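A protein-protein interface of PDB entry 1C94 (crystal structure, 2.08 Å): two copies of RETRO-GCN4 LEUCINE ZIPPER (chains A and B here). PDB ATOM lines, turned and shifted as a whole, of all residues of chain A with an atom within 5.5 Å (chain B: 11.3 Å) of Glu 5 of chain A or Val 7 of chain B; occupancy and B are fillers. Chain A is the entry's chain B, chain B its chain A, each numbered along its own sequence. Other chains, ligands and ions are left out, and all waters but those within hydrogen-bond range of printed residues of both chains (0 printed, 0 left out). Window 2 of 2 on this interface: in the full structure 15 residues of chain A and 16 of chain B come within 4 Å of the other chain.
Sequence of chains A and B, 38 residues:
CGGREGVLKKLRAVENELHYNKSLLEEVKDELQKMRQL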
ATOM      1  N   GLY A   2      -7.287 -25.890  -5.917  1.00  0.00           N
ATOM      2  CA  GLY A   2      -8.059 -24.842  -6.680  1.00  0.00           C
ATOM      3  C   GLY A   2      -8.492 -25.160  -8.119  1.00  0.00           C
ATOM      4  O   GLY A   2      -8.852 -24.231  -8.851  1.00  0.00           O
ATOM      5  N   GLY A   3      -8.497 -26.436  -8.523  1.00  0.00           N
ATOM      6  CA  GLY A   3      -8.862 -26.823  -9.894  1.00  0.00           C
ATOM      7  C   GLY A   3      -9.924 -26.110 -10.753  1.00  0.00           C
ATOM      8  O   GLY A   3      -9.704 -25.016 -11.282  1.00  0.00           O
ATOM      9  N   ARG A   4     -11.051 -26.814 -10.920  1.00  0.00           N
ATOM     10  CA  ARG A   4     -12.320 -26.487 -11.640  1.00  0.00           C
ATOM     11  C   ARG A   4     -13.335 -26.606 -10.480  1.00  0.00           C
ATOM     12  O   ARG A   4     -12.932 -26.509  -9.300  1.00  0.00           O
ATOM     13  CB  ARG A   4     -12.601 -27.606 -12.667  1.00  0.00           C
ATOM     14  CG  ARG A   4     -12.377 -28.973 -12.032  1.00  0.00           C
ATOM     15  CD  ARG A   4     -12.203 -30.134 -13.012  1.00  0.00           C
ATOM     16  NE  ARG A   4     -13.365 -31.039 -13.015  1.00  0.00           N
ATOM     17  CZ  ARG A   4     -13.317 -32.340 -13.304  1.00  0.00           C
ATOM     18  NH1 ARG A   4     -12.158 -32.914 -13.612  1.00  0.00           N
ATOM     19  NH2 ARG A   4     -14.433 -33.067 -13.291  1.00  0.00           N
ATOM     20  N   GLU A   5     -14.624 -26.804 -10.763  1.00  0.00           N
ATOM     21  CA  GLU A   5     -15.519 -27.000  -9.634  1.00  0.00           C
ATOM     22  C   GLU A   5     -16.721 -27.956  -9.765  1.00  0.00           C
ATOM     23  O   GLU A   5     -17.748 -27.692 -10.461  1.00  0.00           O
ATOM     24  CB  GLU A   5     -15.920 -25.658  -9.006  1.00  0.00           C
ATOM     25  CG  GLU A   5     -15.025 -25.284  -7.769  1.00  0.00           C
ATOM     26  CD  GLU A   5     -14.219 -23.950  -7.892  1.00  0.00           C
ATOM     27  OE1 GLU A   5     -14.039 -23.422  -9.004  1.00  0.00           O
ATOM     28  OE2 GLU A   5     -13.736 -23.426  -6.859  1.00  0.00           O
ATOM     29  N   GLY A   6     -16.509 -29.126  -9.129  1.00  0.00           N
ATOM     30  CA  GLY A   6     -17.542 -30.147  -8.993  1.00  0.00           C
ATOM     31  C   GLY A   6     -18.255 -29.591  -7.774  1.00  0.00           C
ATOM     32  O   GLY A   6     -19.419 -29.813  -7.530  1.00  0.00           O
ATOM     33  N   VAL A   7     -17.544 -28.764  -7.033  1.00  0.00           N
ATOM     34  CA  VAL A   7     -18.137 -28.118  -5.888  1.00  0.00           C
ATOM     35  C   VAL A   7     -19.344 -27.182  -6.214  1.00  0.00           C
ATOM     36  O   VAL A   7     -20.372 -27.117  -5.494  1.00  0.00           O
ATOM     37  CB  VAL A   7     -17.084 -27.361  -5.227  1.00  0.00           C
ATOM     38  CG1 VAL A   7     -17.738 -26.351  -4.221  1.00  0.00           C
ATOM     39  CG2 VAL A   7     -16.238 -28.344  -4.482  1.00  0.00           C
ATOM     40  N   LEU A   8     -19.186 -26.413  -7.273  1.00  0.00           N
ATOM     41  CA  LEU A   8     -20.199 -25.498  -7.736  1.00  0.00           C
ATOM     42  C   LEU A   8     -21.357 -26.355  -8.193  1.00  0.00           C
ATOM     43  O   LEU A   8     -22.565 -26.022  -7.985  1.00  0.00           O
ATOM     44  CB  LEU A   8     -19.662 -24.669  -8.939  1.00  0.00           C
ATOM     45  CG  LEU A   8     -18.945 -23.338  -8.666  1.00  0.00           C
ATOM     46  CD1 LEU A   8     -18.570 -22.598  -9.981  1.00  0.00           C
ATOM     47  CD2 LEU A   8     -19.864 -22.460  -7.790  1.00  0.00           C
ATOM     48  N   LYS A   9     -21.036 -27.451  -8.850  1.00  0.00           N
ATOM     49  CA  LYS A   9     -22.157 -28.266  -9.335  1.00  0.00           C
ATOM     50  C   LYS A   9     -22.964 -28.795  -8.195  1.00  0.00           C
ATOM     51  O   LYS A   9     -24.181 -28.890  -8.279  1.00  0.00           O
ATOM     52  CB  LYS A   9     -21.667 -29.414 -10.206  1.00  0.00           C
ATOM     53  CG  LYS A   9     -22.775 -30.438 -10.565  1.00  0.00           C
ATOM     54  CD  LYS A   9     -22.268 -31.700 -11.314  1.00  0.00           C
ATOM     55  CE  LYS A   9     -21.559 -32.706 -10.371  1.00  0.00           C
ATOM     56  NZ  LYS A   9     -21.328 -34.091 -10.964  1.00  0.00           N
ATOM     57  N   LEU A  11     -23.140 -27.415  -5.220  1.00  0.00           N
ATOM     58  CA  LEU A  11     -23.856 -26.318  -4.535  1.00  0.00           C
ATOM     59  C   LEU A  11     -25.114 -25.945  -5.364  1.00  0.00           C
ATOM     60  O   LEU A  11     -26.156 -25.541  -4.872  1.00  0.00           O
ATOM     61  CB  LEU A  11     -22.910 -25.137  -4.466  1.00  0.00           C
ATOM     62  CG  LEU A  11     -21.969 -25.203  -3.251  1.00  0.00           C
ATOM     63  CD1 LEU A  11     -21.091 -24.026  -3.542  1.00  0.00           C
ATOM     64  CD2 LEU A  11     -22.831 -24.835  -1.917  1.00  0.00           C
ATOM     65  N   GLY B   2      -9.625 -19.740  -8.636  1.00  0.00           N
ATOM     66  CA  GLY B   2      -8.970 -20.798  -7.851  1.00  0.00           C
ATOM     67  C   GLY B   2      -8.378 -20.021  -6.726  1.00  0.00           C
ATOM     68  O   GLY B   2      -7.868 -20.569  -5.750  1.00  0.00           O
ATOM     69  N   GLY B   3      -8.465 -18.707  -6.899  1.00  0.00           N
ATOM     70  CA  GLY B   3      -7.956 -17.781  -5.919  1.00  0.00           C
ATOM     71  C   GLY B   3      -9.090 -16.944  -5.360  1.00  0.00           C
ATOM     72  O   GLY B   3      -8.951 -16.314  -4.300  1.00  0.00           O
ATOM     73  N   ARG B   4     -10.240 -16.936  -6.037  1.00  0.00           N
ATOM     74  CA  ARG B   4     -11.337 -16.113  -5.511  1.00  0.00           C
ATOM     75  C   ARG B   4     -12.489 -17.041  -5.149  1.00  0.00           C
ATOM     76  O   ARG B   4     -12.307 -18.268  -5.127  1.00  0.00           O
ATOM     77  CB  ARG B   4     -11.784 -15.110  -6.577  1.00  0.00           C
ATOM     78  CG  ARG B   4     -12.214 -15.818  -7.849  1.00  0.00           C
ATOM     79  CD  ARG B   4     -12.325 -14.907  -9.061  1.00  0.00           C
ATOM     80  NE  ARG B   4     -13.715 -14.626  -9.426  1.00  0.00           N
ATOM     81  CZ  ARG B   4     -14.128 -14.358 -10.663  1.00  0.00           C
ATOM     82  NH1 ARG B   4     -13.260 -14.335 -11.671  1.00  0.00           N
ATOM     83  NH2 ARG B   4     -15.412 -14.117 -10.896  1.00  0.00           N
ATOM     84  N   GLU B   5     -13.664 -16.484  -4.839  1.00  0.00           N
ATOM     85  CA  GLU B   5     -14.767 -17.373  -4.564  1.00  0.00           C
ATOM     86  C   GLU B   5     -16.177 -16.988  -4.994  1.00  0.00           C
ATOM     87  O   GLU B   5     -16.861 -16.108  -4.412  1.00  0.00           O
ATOM     88  CB  GLU B   5     -14.719 -17.875  -3.109  1.00  0.00           C
ATOM     89  CG  GLU B   5     -14.032 -19.287  -2.991  1.00  0.00           C
ATOM     90  CD  GLU B   5     -12.746 -19.348  -2.112  1.00  0.00           C
ATOM     91  OE1 GLU B   5     -12.159 -18.297  -1.793  1.00  0.00           O
ATOM     92  OE2 GLU B   5     -12.297 -20.458  -1.742  1.00  0.00           O
ATOM     93  N   GLY B   6     -16.566 -17.643  -6.095  1.00  0.00           N
ATOM     94  CA  GLY B   6     -17.915 -17.545  -6.639  1.00  0.00           C
ATOM     95  C   GLY B   6     -18.568 -18.598  -5.754  1.00  0.00           C
ATOM     96  O   GLY B   6     -19.766 -18.607  -5.521  1.00  0.00           O
ATOM     97  N   VAL B   7     -17.731 -19.459  -5.157  1.00  0.00           N
ATOM     98  CA  VAL B   7     -18.268 -20.453  -4.242  1.00  0.00           C
ATOM     99  C   VAL B   7     -18.936 -19.820  -2.993  1.00  0.00           C
ATOM    100  O   VAL B   7     -20.020 -20.192  -2.549  1.00  0.00           O
ATOM    101  CB  VAL B   7     -17.206 -21.306  -3.827  1.00  0.00           C
ATOM    102  CG1 VAL B   7     -17.698 -22.173  -2.643  1.00  0.00           C
ATOM    103  CG2 VAL B   7     -16.847 -22.265  -5.025  1.00  0.00           C
ATOM    104  N   LEU B   8     -18.250 -18.866  -2.429  1.00  0.00           N
ATOM    105  CA  LEU B   8     -18.696 -18.154  -1.274  1.00  0.00           C
ATOM    106  C   LEU B   8     -19.954 -17.466  -1.644  1.00  0.00           C
ATOM    107  O   LEU B   8     -20.903 -17.432  -0.815  1.00  0.00           O
ATOM    108  CB  LEU B   8     -17.630 -17.099  -0.853  1.00  0.00           C
ATOM    109  CG  LEU B   8     -16.562 -17.530   0.144  1.00  0.00           C
ATOM    110  CD1 LEU B   8     -15.698 -16.289   0.584  1.00  0.00           C
ATOM    111  CD2 LEU B   8     -17.207 -18.186   1.321  1.00  0.00           C
ATOM    112  N   LYS B   9     -19.990 -16.864  -2.832  1.00  0.00           N
ATOM    113  CA  LYS B   9     -21.201 -16.184  -3.175  1.00  0.00           C
ATOM    114  C   LYS B   9     -22.384 -17.108  -3.225  1.00  0.00           C
ATOM    115  O   LYS B   9     -23.489 -16.706  -2.847  1.00  0.00           O
ATOM    116  CB  LYS B   9     -21.060 -15.422  -4.526  1.00  0.00           C
ATOM    117  CG  LYS B   9     -22.359 -14.841  -5.070  1.00  0.00           C
ATOM    118  CD  LYS B   9     -22.288 -14.231  -6.497  1.00  0.00           C
ATOM    119  CE  LYS B   9     -22.255 -15.333  -7.634  1.00  0.00           C
ATOM    120  NZ  LYS B   9     -22.466 -14.836  -9.048  1.00  0.00           N
ATOM    121  N   LYS B  10     -22.187 -18.291  -3.814  1.00  0.00           N
ATOM    122  CA  LYS B  10     -23.221 -19.310  -3.935  1.00  0.00           C
ATOM    123  C   LYS B  10     -23.627 -19.777  -2.542  1.00  0.00           C
ATOM    124  O   LYS B  10     -24.781 -19.822  -2.184  1.00  0.00           O
ATOM    125  CB  LYS B  10     -22.632 -20.425  -4.798  1.00  0.00           C
ATOM    126  CG  LYS B  10     -23.448 -21.684  -5.071  1.00  0.00           C
ATOM    127  CD  LYS B  10     -24.500 -21.572  -6.207  1.00  0.00           C
ATOM    128  CE  LYS B  10     -24.429 -22.798  -7.150  1.00  0.00           C
ATOM    129  NZ  LYS B  10     -22.994 -23.109  -7.763  1.00  0.00           N
ATOM    130  N   LEU B  11     -22.676 -19.980  -1.663  1.00  0.00           N
ATOM    131  CA  LEU B  11     -23.003 -20.440  -0.289  1.00  0.00           C
ATOM    132  C   LEU B  11     -23.773 -19.365   0.477  1.00  0.00           C
ATOM    133  O   LEU B  11     -24.616 -19.652   1.370  1.00  0.00           O
ATOM    134  CB  LEU B  11     -21.689 -20.678   0.446  1.00  0.00           C
ATOM    135  CG  LEU B  11     -21.150 -22.070   0.252  1.00  0.00           C
ATOM    136  CD1 LEU B  11     -19.865 -22.077   1.008  1.00  0.00           C
ATOM    137  CD2 LEU B  11     -22.085 -23.094   0.939  1.00  0.00           C
ATOM    138  N   ARG B  12     -23.560 -18.086   0.136  1.00  0.00           N
ATOM    139  CA  ARG B  12     -24.222 -17.015   0.858  1.00  0.00           C
ATOM    140  C   ARG B  12     -25.704 -16.982   0.428  1.00  0.00           C
ATOM    141  O   ARG B  12     -26.554 -16.849   1.238  1.00  0.00           O
ATOM    142  CB  ARG B  12     -23.403 -15.711   0.619  1.00  0.00           C
ATOM    143  CG  ARG B  12     -23.585 -14.561   1.654  1.00  0.00           C
ATOM    144  CD  ARG B  12     -23.170 -13.131   1.051  1.00  0.00           C
ATOM    145  NE  ARG B  12     -21.885 -13.095   0.278  1.00  0.00           N
ATOM    146  CZ  ARG B  12     -20.724 -13.696   0.616  1.00  0.00           C
ATOM    147  NH1 ARG B  12     -20.559 -14.429   1.748  1.00  0.00           N
ATOM    148  NH2 ARG B  12     -19.710 -13.611  -0.236  1.00  0.00           N
ATOM    149  N   ALA B  13     -25.992 -17.134  -0.868  1.00  0.00           N
ATOM    150  CA  ALA B  13     -27.339 -17.246  -1.373  1.00  0.00           C
ATOM    151  C   ALA B  13     -28.009 -18.489  -0.704  1.00  0.00           C
ATOM    152  O   ALA B  13     -29.173 -18.460  -0.270  1.00  0.00           O
ATOM    153  CB  ALA B  13     -27.259 -17.482  -2.970  1.00  0.00           C
ATOM    154  N   VAL B  14     -27.277 -19.583  -0.633  1.00  0.00           N
ATOM    155  CA  VAL B  14     -27.797 -20.811   0.030  1.00  0.00           C
ATOM    156  C   VAL B  14     -28.202 -20.565   1.467  1.00  0.00           C
ATOM    157  O   VAL B  14     -29.266 -20.950   1.943  1.00  0.00           O
ATOM    158  CB  VAL B  14     -26.680 -21.943  -0.007  1.00  0.00           C
ATOM    159  CG1 VAL B  14     -26.965 -23.127   1.058  1.00  0.00           C
ATOM    160  CG2 VAL B  14     -26.735 -22.625  -1.319  1.00  0.00           C
ATOM    161  N   GLU B  15     -27.284 -20.015   2.244  1.00  0.00           N
ATOM    162  CA  GLU B  15     -27.592 -19.707   3.617  1.00  0.00           C
ATOM    163  C   GLU B  15     -28.725 -18.694   3.735  1.00  0.00           C
ATOM    164  O   GLU B  15     -29.625 -18.873   4.610  1.00  0.00           O
ATOM    165  CB  GLU B  15     -26.209 -19.276   4.388  1.00  0.00           C
ATOM    166  CG  GLU B  15     -26.402 -19.002   5.934  1.00  0.00           C
ATOM    167  CD  GLU B  15     -27.273 -17.888   6.363  1.00  0.00           C
ATOM    168  OE1 GLU B  15     -27.262 -16.804   5.742  1.00  0.00           O
ATOM    169  OE2 GLU B  15     -27.960 -18.077   7.399  1.00  0.00           O
ATOM    170  N   ASN B  16     -28.786 -17.643   2.863  1.00  0.00           N
ATOM    171  CA  ASN B  16     -29.954 -16.739   2.959  1.00  0.00           C
ATOM    172  C   ASN B  16     -31.308 -17.513   2.690  1.00  0.00           C
ATOM    173  O   ASN B  16     -32.360 -17.324   3.354  1.00  0.00           O
ATOM    174  CB  ASN B  16     -29.734 -15.558   1.921  1.00  0.00           C
ATOM    175  CG  ASN B  16     -28.754 -14.472   2.495  1.00  0.00           C
ATOM    176  OD1 ASN B  16     -28.663 -14.379   3.685  1.00  0.00           O
ATOM    177  ND2 ASN B  16     -28.018 -13.739   1.669  1.00  0.00           N
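The side-chain amino group (NZ) of Lys 10 of chain B lies within hydrogen-bond range of the backbone carbonyl oxygen (O) of Leu 8 of chain A (3.0 Å).
Among the printed residues, merely in contact across the chains: Leu 11 of chain A with Leu 11 of chain B (3.4 Å), Leu 11 of chain A with Lys 10 of chain B (3.5 Å), Gly 2 of chain A with Gly 2 of chain B (3.6 Å), Glu 5 of chain A with Val 7 of chain B (3.8 Å) and Leu 11 of chain A with Val 7 of chain B (3.97 Å).
Gly 2 of chain A touches just one residue of chain B: Gly 2 (3.6 Å). No residue of chain B comes within 4 Å of Gly 3 of chain A. Glu 5 of chain A touches just one residue of chain B: Val 7. No residue of chain B comes within 4 Å of Gly 6 of chain A. No residue of chain B comes within 4 Å of Val 7 of chain A. Leu 8 of chain A touches just one residue of chain B: Lys 10. Printed residues of chain B within 4 Å of Leu 11 of chain A: Val 7 (3.97 Å), Lys 10 (3.5 Å) and Leu 11 (3.4 Å). Of the printed residues of chain A, Gly 2 of chain B touches Gly 2. Of the printed residues of chain A, Val 7 of chain B touches Glu 5 and Leu 11. Leu 8 of chain B touches none of the printed residues of chain A. Of the printed residues of chain A, Leu 11 of chain B touches Leu 11. The nearest residue of chain B that does not touch Glu 5 of chain A is Gly 2 of chain B (5.5 Å). The nearest printed residue of chain A that does not touch Gly 2 of chain B is Gly 3 of chain A (5.5 Å).
Hydrophobic or aromatic side chains of chain A that line the printed part of chain B: Leu 8 and Leu 11. Along chain B the printed residues that touch a printed residue of chain A span positions 2 to 11. Among the printed residues, 6 pairs touch across the chains.
Gly 2 of chain B touches its own counterpart, Gly 2 of chain A. Glu 5 of chain A touches Val 7 of chain B, but with the chains exchanged Val 7 of chain A does not touch Glu 5 of chain B (8.1 Å). Leu 11 of chain A touches Val 7 of chain B, but with the chains exchanged Val 7 of chain A does not touch Leu 11 of chain B (7.1 Å). Leu 11 of chain B touches its own counterpart, Leu 11 of chain A. Positions printed for both chains: 2, 3, 4, 5, 6, 7, 8, 9 and 11. Of the 6 pairs that touch across the chains among the printed residues, 2 have their exchanged pair printed and touching as well.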
